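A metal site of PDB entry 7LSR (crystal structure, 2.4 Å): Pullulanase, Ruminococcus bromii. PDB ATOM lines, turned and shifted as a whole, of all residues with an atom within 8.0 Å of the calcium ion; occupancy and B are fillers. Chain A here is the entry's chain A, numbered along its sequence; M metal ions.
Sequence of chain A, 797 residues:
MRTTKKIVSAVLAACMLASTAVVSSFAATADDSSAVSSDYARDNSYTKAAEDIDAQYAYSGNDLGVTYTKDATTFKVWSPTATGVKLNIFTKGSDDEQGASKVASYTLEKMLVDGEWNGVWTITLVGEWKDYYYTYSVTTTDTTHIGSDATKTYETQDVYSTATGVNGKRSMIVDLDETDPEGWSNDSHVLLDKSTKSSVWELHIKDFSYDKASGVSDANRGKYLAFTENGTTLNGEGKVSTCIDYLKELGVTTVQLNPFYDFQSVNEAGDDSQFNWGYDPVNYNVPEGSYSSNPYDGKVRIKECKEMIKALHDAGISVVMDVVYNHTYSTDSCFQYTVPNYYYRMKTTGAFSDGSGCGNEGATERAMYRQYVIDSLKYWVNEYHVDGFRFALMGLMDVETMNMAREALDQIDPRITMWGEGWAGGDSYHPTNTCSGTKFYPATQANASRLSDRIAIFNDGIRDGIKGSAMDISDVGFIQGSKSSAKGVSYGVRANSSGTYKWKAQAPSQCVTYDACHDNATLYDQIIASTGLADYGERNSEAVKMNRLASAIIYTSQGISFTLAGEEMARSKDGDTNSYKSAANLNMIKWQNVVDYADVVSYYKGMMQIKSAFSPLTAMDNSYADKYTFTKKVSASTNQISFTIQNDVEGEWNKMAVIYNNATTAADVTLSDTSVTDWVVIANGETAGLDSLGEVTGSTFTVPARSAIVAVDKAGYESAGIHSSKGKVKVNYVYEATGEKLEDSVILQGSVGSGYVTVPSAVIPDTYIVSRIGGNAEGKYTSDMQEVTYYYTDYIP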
ATOM      1  N   THR A 164      35.710 -13.383 -10.804  1.00  0.00           N
ATOM      2  CA  THR A 164      36.263 -14.431 -11.668  1.00  0.00           C
ATOM      3  C   THR A 164      35.687 -14.307 -13.080  1.00  0.00           C
ATOM      4  O   THR A 164      34.695 -13.600 -13.300  1.00  0.00           O
ATOM      5  CB  THR A 164      35.979 -15.832 -11.126  1.00  0.00           C
ATOM      6  OG1 THR A 164      34.561 -16.011 -11.093  1.00  0.00           O
ATOM      7  CG2 THR A 164      36.556 -16.085  -9.761  1.00  0.00           C
ATOM      8  N   GLY A 165      36.313 -15.029 -14.022  1.00  0.00           N
ATOM      9  CA  GLY A 165      35.796 -15.195 -15.375  1.00  0.00           C
ATOM     10  C   GLY A 165      34.720 -16.263 -15.428  1.00  0.00           C
ATOM     11  O   GLY A 165      34.091 -16.567 -14.405  1.00  0.00           O
ATOM     12  N   VAL A 166      34.505 -16.834 -16.613  1.00  0.00           N
ATOM     13  CA  VAL A 166      33.475 -17.855 -16.831  1.00  0.00           C
ATOM     14  C   VAL A 166      33.904 -19.150 -16.117  1.00  0.00           C
ATOM     15  O   VAL A 166      35.051 -19.600 -16.257  1.00  0.00           O
ATOM     16  CB  VAL A 166      33.209 -18.077 -18.334  1.00  0.00           C
ATOM     17  CG1 VAL A 166      34.372 -18.736 -19.058  1.00  0.00           C
ATOM     18  CG2 VAL A 166      31.922 -18.859 -18.562  1.00  0.00           C
ATOM     19  N   ASN A 167      32.989 -19.695 -15.317  1.00  0.00           N
ATOM     20  CA  ASN A 167      33.125 -20.988 -14.612  1.00  0.00           C
ATOM     21  C   ASN A 167      34.205 -20.907 -13.518  1.00  0.00           C
ATOM     22  O   ASN A 167      34.721 -21.937 -13.093  1.00  0.00           O
ATOM     23  CB  ASN A 167      33.373 -22.146 -15.591  1.00  0.00           C
ATOM     24  CG  ASN A 167      32.203 -22.398 -16.519  1.00  0.00           C
ATOM     25  OD1 ASN A 167      31.043 -22.183 -16.149  1.00  0.00           O
ATOM     26  ND2 ASN A 167      32.488 -22.852 -17.721  1.00  0.00           N
ATOM     27  N   GLY A 168      34.508 -19.682 -13.059  1.00  0.00           N
ATOM     28  CA  GLY A 168      35.303 -19.436 -11.852  1.00  0.00           C
ATOM     29  C   GLY A 168      36.599 -20.227 -11.782  1.00  0.00           C
ATOM     30  O   GLY A 168      36.916 -20.800 -10.736  1.00  0.00           O
ATOM     31  N   TYR A 261      26.040 -17.199  -4.638  1.00  0.00           N
ATOM     32  CA  TYR A 261      27.496 -17.402  -4.688  1.00  0.00           C
ATOM     33  C   TYR A 261      27.789 -18.294  -5.900  1.00  0.00           C
ATOM     34  O   TYR A 261      26.880 -18.948  -6.407  1.00  0.00           O
ATOM     35  CB  TYR A 261      28.010 -18.018  -3.381  1.00  0.00           C
ATOM     36  CG  TYR A 261      27.415 -19.366  -3.065  1.00  0.00           C
ATOM     37  CD1 TYR A 261      27.927 -20.520  -3.640  1.00  0.00           C
ATOM     38  CD2 TYR A 261      26.337 -19.493  -2.212  1.00  0.00           C
ATOM     39  CE1 TYR A 261      27.378 -21.761  -3.376  1.00  0.00           C
ATOM     40  CE2 TYR A 261      25.774 -20.731  -1.929  1.00  0.00           C
ATOM     41  CZ  TYR A 261      26.292 -21.866  -2.517  1.00  0.00           C
ATOM     42  OH  TYR A 261      25.762 -23.093  -2.263  1.00  0.00           O
ATOM     43  N   ASP A 262      29.051 -18.324  -6.351  1.00  0.00           N
ATOM     44  CA  ASP A 262      29.409 -19.072  -7.568  1.00  0.00           C
ATOM     45  C   ASP A 262      29.454 -20.575  -7.252  1.00  0.00           C
ATOM     46  O   ASP A 262      30.160 -21.004  -6.346  1.00  0.00           O
ATOM     47  CB  ASP A 262      30.739 -18.590  -8.151  1.00  0.00           C
ATOM     48  CG  ASP A 262      31.060 -19.189  -9.502  1.00  0.00           C
ATOM     49  OD1 ASP A 262      30.110 -19.457 -10.276  1.00  0.00           O
ATOM     50  OD2 ASP A 262      32.262 -19.382  -9.793  1.00  0.00           O
ATOM     51  N   PHE A 263      28.709 -21.355  -8.047  1.00  0.00           N
ATOM     52  CA  PHE A 263      28.640 -22.813  -7.918  1.00  0.00           C
ATOM     53  C   PHE A 263      28.993 -23.474  -9.264  1.00  0.00           C
ATOM     54  O   PHE A 263      29.075 -22.796 -10.284  1.00  0.00           O
ATOM     55  CB  PHE A 263      27.263 -23.250  -7.402  1.00  0.00           C
ATOM     56  CG  PHE A 263      26.083 -22.678  -8.156  1.00  0.00           C
ATOM     57  CD1 PHE A 263      25.571 -23.322  -9.274  1.00  0.00           C
ATOM     58  CD2 PHE A 263      25.465 -21.514  -7.718  1.00  0.00           C
ATOM     59  CE1 PHE A 263      24.482 -22.800  -9.955  1.00  0.00           C
ATOM     60  CE2 PHE A 263      24.371 -20.994  -8.412  1.00  0.00           C
ATOM     61  CZ  PHE A 263      23.892 -21.636  -9.528  1.00  0.00           C
ATOM     62  N   GLN A 264      29.189 -24.794  -9.232  1.00  0.00           N
ATOM     63  CA  GLN A 264      29.772 -25.565 -10.340  1.00  0.00           C
ATOM     64  C   GLN A 264      28.695 -26.044 -11.319  1.00  0.00           C
ATOM     65  O   GLN A 264      28.944 -26.127 -12.526  1.00  0.00           O
ATOM     66  CB  GLN A 264      30.532 -26.770  -9.772  1.00  0.00           C
ATOM     67  CG  GLN A 264      31.187 -27.659 -10.827  1.00  0.00           C
ATOM     68  CD  GLN A 264      30.291 -28.764 -11.328  1.00  0.00           C
ATOM     69  OE1 GLN A 264      29.276 -29.106 -10.717  1.00  0.00           O
ATOM     70  NE2 GLN A 264      30.654 -29.347 -12.461  1.00  0.00           N
ATOM     71  N   SER A 265      27.495 -26.337 -10.798  1.00  0.00           N
ATOM     72  CA  SER A 265      26.545 -27.269 -11.424  1.00  0.00           C
ATOM     73  C   SER A 265      25.801 -26.668 -12.631  1.00  0.00           C
ATOM     74  O   SER A 265      24.966 -27.361 -13.221  1.00  0.00           O
ATOM     75  CB  SER A 265      25.583 -27.786 -10.387  1.00  0.00           C
ATOM     76  OG  SER A 265      25.099 -26.727  -9.568  1.00  0.00           O
ATOM     77  N   VAL A 266      26.077 -25.410 -12.991  1.00  0.00           N
ATOM     78  CA  VAL A 266      25.585 -24.827 -14.240  1.00  0.00           C
ATOM     79  C   VAL A 266      26.792 -24.385 -15.082  1.00  0.00           C
ATOM     80  O   VAL A 266      27.635 -23.625 -14.615  1.00  0.00           O
ATOM     81  CB  VAL A 266      24.611 -23.666 -14.000  1.00  0.00           C
ATOM     82  CG1 VAL A 266      24.354 -22.854 -15.266  1.00  0.00           C
ATOM     83  CG2 VAL A 266      23.295 -24.145 -13.409  1.00  0.00           C
ATOM     84  N   ASN A 267      26.843 -24.877 -16.332  1.00  0.00           N
ATOM     85  CA  ASN A 267      27.809 -24.426 -17.328  1.00  0.00           C
ATOM     86  C   ASN A 267      27.387 -23.029 -17.808  1.00  0.00           C
ATOM     87  O   ASN A 267      26.345 -22.868 -18.429  1.00  0.00           O
ATOM     88  CB  ASN A 267      27.927 -25.417 -18.485  1.00  0.00           C
ATOM     89  CG  ASN A 267      28.959 -25.014 -19.529  1.00  0.00           C
ATOM     90  OD1 ASN A 267      29.610 -23.986 -19.404  1.00  0.00           O
ATOM     91  ND2 ASN A 267      29.108 -25.826 -20.561  1.00  0.00           N
ATOM     92  N   GLU A 268      28.228 -22.029 -17.497  1.00  0.00           N
ATOM     93  CA  GLU A 268      27.909 -20.614 -17.713  1.00  0.00           C
ATOM     94  C   GLU A 268      28.030 -20.245 -19.195  1.00  0.00           C
ATOM     95  O   GLU A 268      27.516 -19.207 -19.615  1.00  0.00           O
ATOM     96  CB  GLU A 268      28.797 -19.735 -16.830  1.00  0.00           C
ATOM     97  CG  GLU A 268      28.489 -19.868 -15.348  1.00  0.00           C
ATOM     98  CD  GLU A 268      29.475 -19.180 -14.423  1.00  0.00           C
ATOM     99  OE1 GLU A 268      30.403 -18.506 -14.920  1.00  0.00           O
ATOM    100  OE2 GLU A 268      29.326 -19.325 -13.193  1.00  0.00           O
ATOM    101  N   ASP A 280      26.568 -26.231  -4.506  1.00  0.00           N
ATOM    102  CA  ASP A 280      27.775 -26.839  -5.064  1.00  0.00           C
ATOM    103  C   ASP A 280      28.872 -25.771  -5.150  1.00  0.00           C
ATOM    104  O   ASP A 280      29.323 -25.442  -6.246  1.00  0.00           O
ATOM    105  CB  ASP A 280      27.487 -27.450  -6.436  1.00  0.00           C
ATOM    106  CG  ASP A 280      26.300 -28.402  -6.451  1.00  0.00           C
ATOM    107  OD1 ASP A 280      26.296 -29.357  -5.658  1.00  0.00           O
ATOM    108  OD2 ASP A 280      25.380 -28.174  -7.262  1.00  0.00           O
ATOM    109  N   VAL A 282      32.043 -23.105  -5.291  1.00  0.00           N
ATOM    110  CA  VAL A 282      33.335 -23.049  -5.975  1.00  0.00           C
ATOM    111  C   VAL A 282      34.088 -21.796  -5.490  1.00  0.00           C
ATOM    112  O   VAL A 282      35.221 -21.892  -5.025  1.00  0.00           O
ATOM    113  CB  VAL A 282      33.159 -23.044  -7.508  1.00  0.00           C
ATOM    114  CG1 VAL A 282      34.477 -22.853  -8.243  1.00  0.00           C
ATOM    115  CG2 VAL A 282      32.458 -24.297  -7.998  1.00  0.00           C
ATOM    116  N   ASN A 283      33.450 -20.625  -5.631  1.00  0.00           N
ATOM    117  CA  ASN A 283      33.957 -19.352  -5.145  1.00  0.00           C
ATOM    118  C   ASN A 283      32.904 -18.721  -4.220  1.00  0.00           C
ATOM    119  O   ASN A 283      31.805 -18.377  -4.666  1.00  0.00           O
ATOM    120  CB  ASN A 283      34.306 -18.404  -6.294  1.00  0.00           C
ATOM    121  CG  ASN A 283      35.346 -18.987  -7.230  1.00  0.00           C
ATOM    122  OD1 ASN A 283      36.463 -19.301  -6.820  1.00  0.00           O
ATOM    123  ND2 ASN A 283      34.989 -19.140  -8.502  1.00  0.00           N
ATOM    124  N   VAL A 286      32.118 -14.640  -4.637  1.00  0.00           N
ATOM    125  CA  VAL A 286      31.907 -14.271  -6.034  1.00  0.00           C
ATOM    126  C   VAL A 286      30.468 -14.608  -6.404  1.00  0.00           C
ATOM    127  O   VAL A 286      29.998 -15.705  -6.112  1.00  0.00           O
ATOM    128  CB  VAL A 286      32.899 -14.999  -6.973  1.00  0.00           C
ATOM    129  CG1 VAL A 286      32.677 -14.639  -8.426  1.00  0.00           C
ATOM    130  CG2 VAL A 286      34.346 -14.743  -6.576  1.00  0.00           C
ATOM    131  N   PRO A 287      29.714 -13.687  -7.048  1.00  0.00           N
ATOM    132  CA  PRO A 287      28.381 -14.008  -7.562  1.00  0.00           C
ATOM    133  C   PRO A 287      28.384 -15.148  -8.594  1.00  0.00           C
ATOM    134  O   PRO A 287      29.394 -15.399  -9.239  1.00  0.00           O
ATOM    135  CB  PRO A 287      27.913 -12.702  -8.239  1.00  0.00           C
ATOM    136  CG  PRO A 287      28.758 -11.619  -7.591  1.00  0.00           C
ATOM    137  CD  PRO A 287      30.082 -12.286  -7.292  1.00  0.00           C
ATOM    138  N   GLU A 288      27.231 -15.817  -8.733  1.00  0.00           N
ATOM    139  CA  GLU A 288      27.031 -16.837  -9.769  1.00  0.00           C
ATOM    140  C   GLU A 288      26.977 -16.134 -11.141  1.00  0.00           C
ATOM    141  O   GLU A 288      26.394 -15.060 -11.270  1.00  0.00           O
ATOM    142  CB  GLU A 288      25.758 -17.637  -9.491  1.00  0.00           C
ATOM    143  CG  GLU A 288      25.315 -18.541 -10.636  1.00  0.00           C
ATOM    144  CD  GLU A 288      26.287 -19.640 -11.024  1.00  0.00           C
ATOM    145  OE1 GLU A 288      27.184 -19.962 -10.211  1.00  0.00           O
ATOM    146  OE2 GLU A 288      26.156 -20.174 -12.133  1.00  0.00           O
ATOM    147  N   GLY A 289      27.592 -16.774 -12.146  1.00  0.00           N
ATOM    148  CA  GLY A 289      27.704 -16.233 -13.493  1.00  0.00           C
ATOM    149  C   GLY A 289      26.468 -16.482 -14.343  1.00  0.00           C
ATOM    150  O   GLY A 289      26.119 -15.641 -15.185  1.00  0.00           O
ATOM    151  N   SER A 290      25.815 -17.620 -14.133  1.00  0.00           N
ATOM    152  CA  SER A 290      24.658 -18.059 -14.934  1.00  0.00           C
ATOM    153  C   SER A 290      23.510 -17.037 -14.857  1.00  0.00           C
ATOM    154  O   SER A 290      22.788 -16.858 -15.844  1.00  0.00           O
ATOM    155  CB  SER A 290      24.189 -19.428 -14.510  1.00  0.00           C
ATOM    156  OG  SER A 290      23.660 -19.402 -13.192  1.00  0.00           O
ATOM    157  N   TYR A 291      23.351 -16.392 -13.700  1.00  0.00           N
ATOM    158  CA  TYR A 291      22.251 -15.438 -13.467  1.00  0.00           C
ATOM    159  C   TYR A 291      22.599 -14.042 -14.010  1.00  0.00           C
ATOM    160  O   TYR A 291      21.750 -13.149 -13.957  1.00  0.00           O
ATOM    161  CB  TYR A 291      21.909 -15.369 -11.975  1.00  0.00           C
ATOM    162  CG  TYR A 291      21.524 -16.680 -11.340  1.00  0.00           C
ATOM    163  CD1 TYR A 291      20.651 -17.552 -11.961  1.00  0.00           C
ATOM    164  CD2 TYR A 291      22.020 -17.041 -10.094  1.00  0.00           C
ATOM    165  CE1 TYR A 291      20.289 -18.756 -11.385  1.00  0.00           C
ATOM    166  CE2 TYR A 291      21.665 -18.235  -9.499  1.00  0.00           C
ATOM    167  CZ  TYR A 291      20.803 -19.104 -10.148  1.00  0.00           C
ATOM    168  OH  TYR A 291      20.452 -20.287  -9.572  1.00  0.00           O
ATOM    169  N   PRO A 295      28.893 -13.731 -18.161  1.00  0.00           N
ATOM    170  CA  PRO A 295      29.812 -14.303 -17.166  1.00  0.00           C
ATOM    171  C   PRO A 295      31.299 -14.212 -17.542  1.00  0.00           C
ATOM    172  O   PRO A 295      32.149 -14.472 -16.690  1.00  0.00           O
ATOM    173  CB  PRO A 295      29.355 -15.769 -17.122  1.00  0.00           C
ATOM    174  CG  PRO A 295      28.896 -16.057 -18.539  1.00  0.00           C
ATOM    175  CD  PRO A 295      28.288 -14.753 -19.022  1.00  0.00           C
ATOM    176  N   ARG A 301      28.602  -9.495 -13.574  1.00  0.00           N
ATOM    177  CA  ARG A 301      27.775 -10.242 -12.619  1.00  0.00           C
ATOM    178  C   ARG A 301      27.702  -9.498 -11.274  1.00  0.00           C
ATOM    179  O   ARG A 301      26.690  -9.571 -10.588  1.00  0.00           O
ATOM    180  CB  ARG A 301      28.289 -11.678 -12.452  1.00  0.00           C
ATOM    181  CG  ARG A 301      29.583 -11.808 -11.651  1.00  0.00           C
ATOM    182  CD  ARG A 301      30.021 -13.252 -11.515  1.00  0.00           C
ATOM    183  NE  ARG A 301      30.549 -13.802 -12.749  1.00  0.00           N
ATOM    184  CZ  ARG A 301      31.109 -15.003 -12.865  1.00  0.00           C
ATOM    185  NH1 ARG A 301      31.186 -15.806 -11.815  1.00  0.00           N
ATOM    186  NH2 ARG A 301      31.577 -15.403 -14.040  1.00  0.00           N
HETATM  187 CA    CA M   1      29.142 -21.193 -11.839  1.00  0.00          CA
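OE2 of Glu 268 lies close to N of Gly 289 (3.3 Å).
The side-chain carboxylate (OE1) of Glu 268 is in hydrogen-bond range of the backbone NH (N) of Asn 167.
The side-chain carboxylate of Glu 268 is in salt-bridge range of the guanidinium group of Arg 301, at 3.4 Å.
O of Asp 262 sits at hydrogen-bond distance from N of Val 282 (3.0 Å).
ND2 of Asn 283 sits at hydrogen-bond distance from OD2 of Asp 262, at 3.0 Å.
The backbone NH of Asp 262 lies within hydrogen-bond range of the backbone carbonyl oxygen of Val 286, at 2.8 Å.
OE2 of Glu 288 lies within hydrogen-bond range of OG of Ser 290 (2.8 Å).
Val 266 touches the calcium ion.
The backbone carbonyl oxygen (O) of Phe 263 is bound to the calcium ion.
The calcium ion is bound by OE2 of Glu 268 (2.3 Å).
The calcium ion is bound by the side-chain carboxylate (OD1) of Asp 262 (2.5 Å).
OE1 of Glu 288 is bound to the calcium ion, at 2.8 Å.
The calcium ion has four donor atoms within binding distance.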
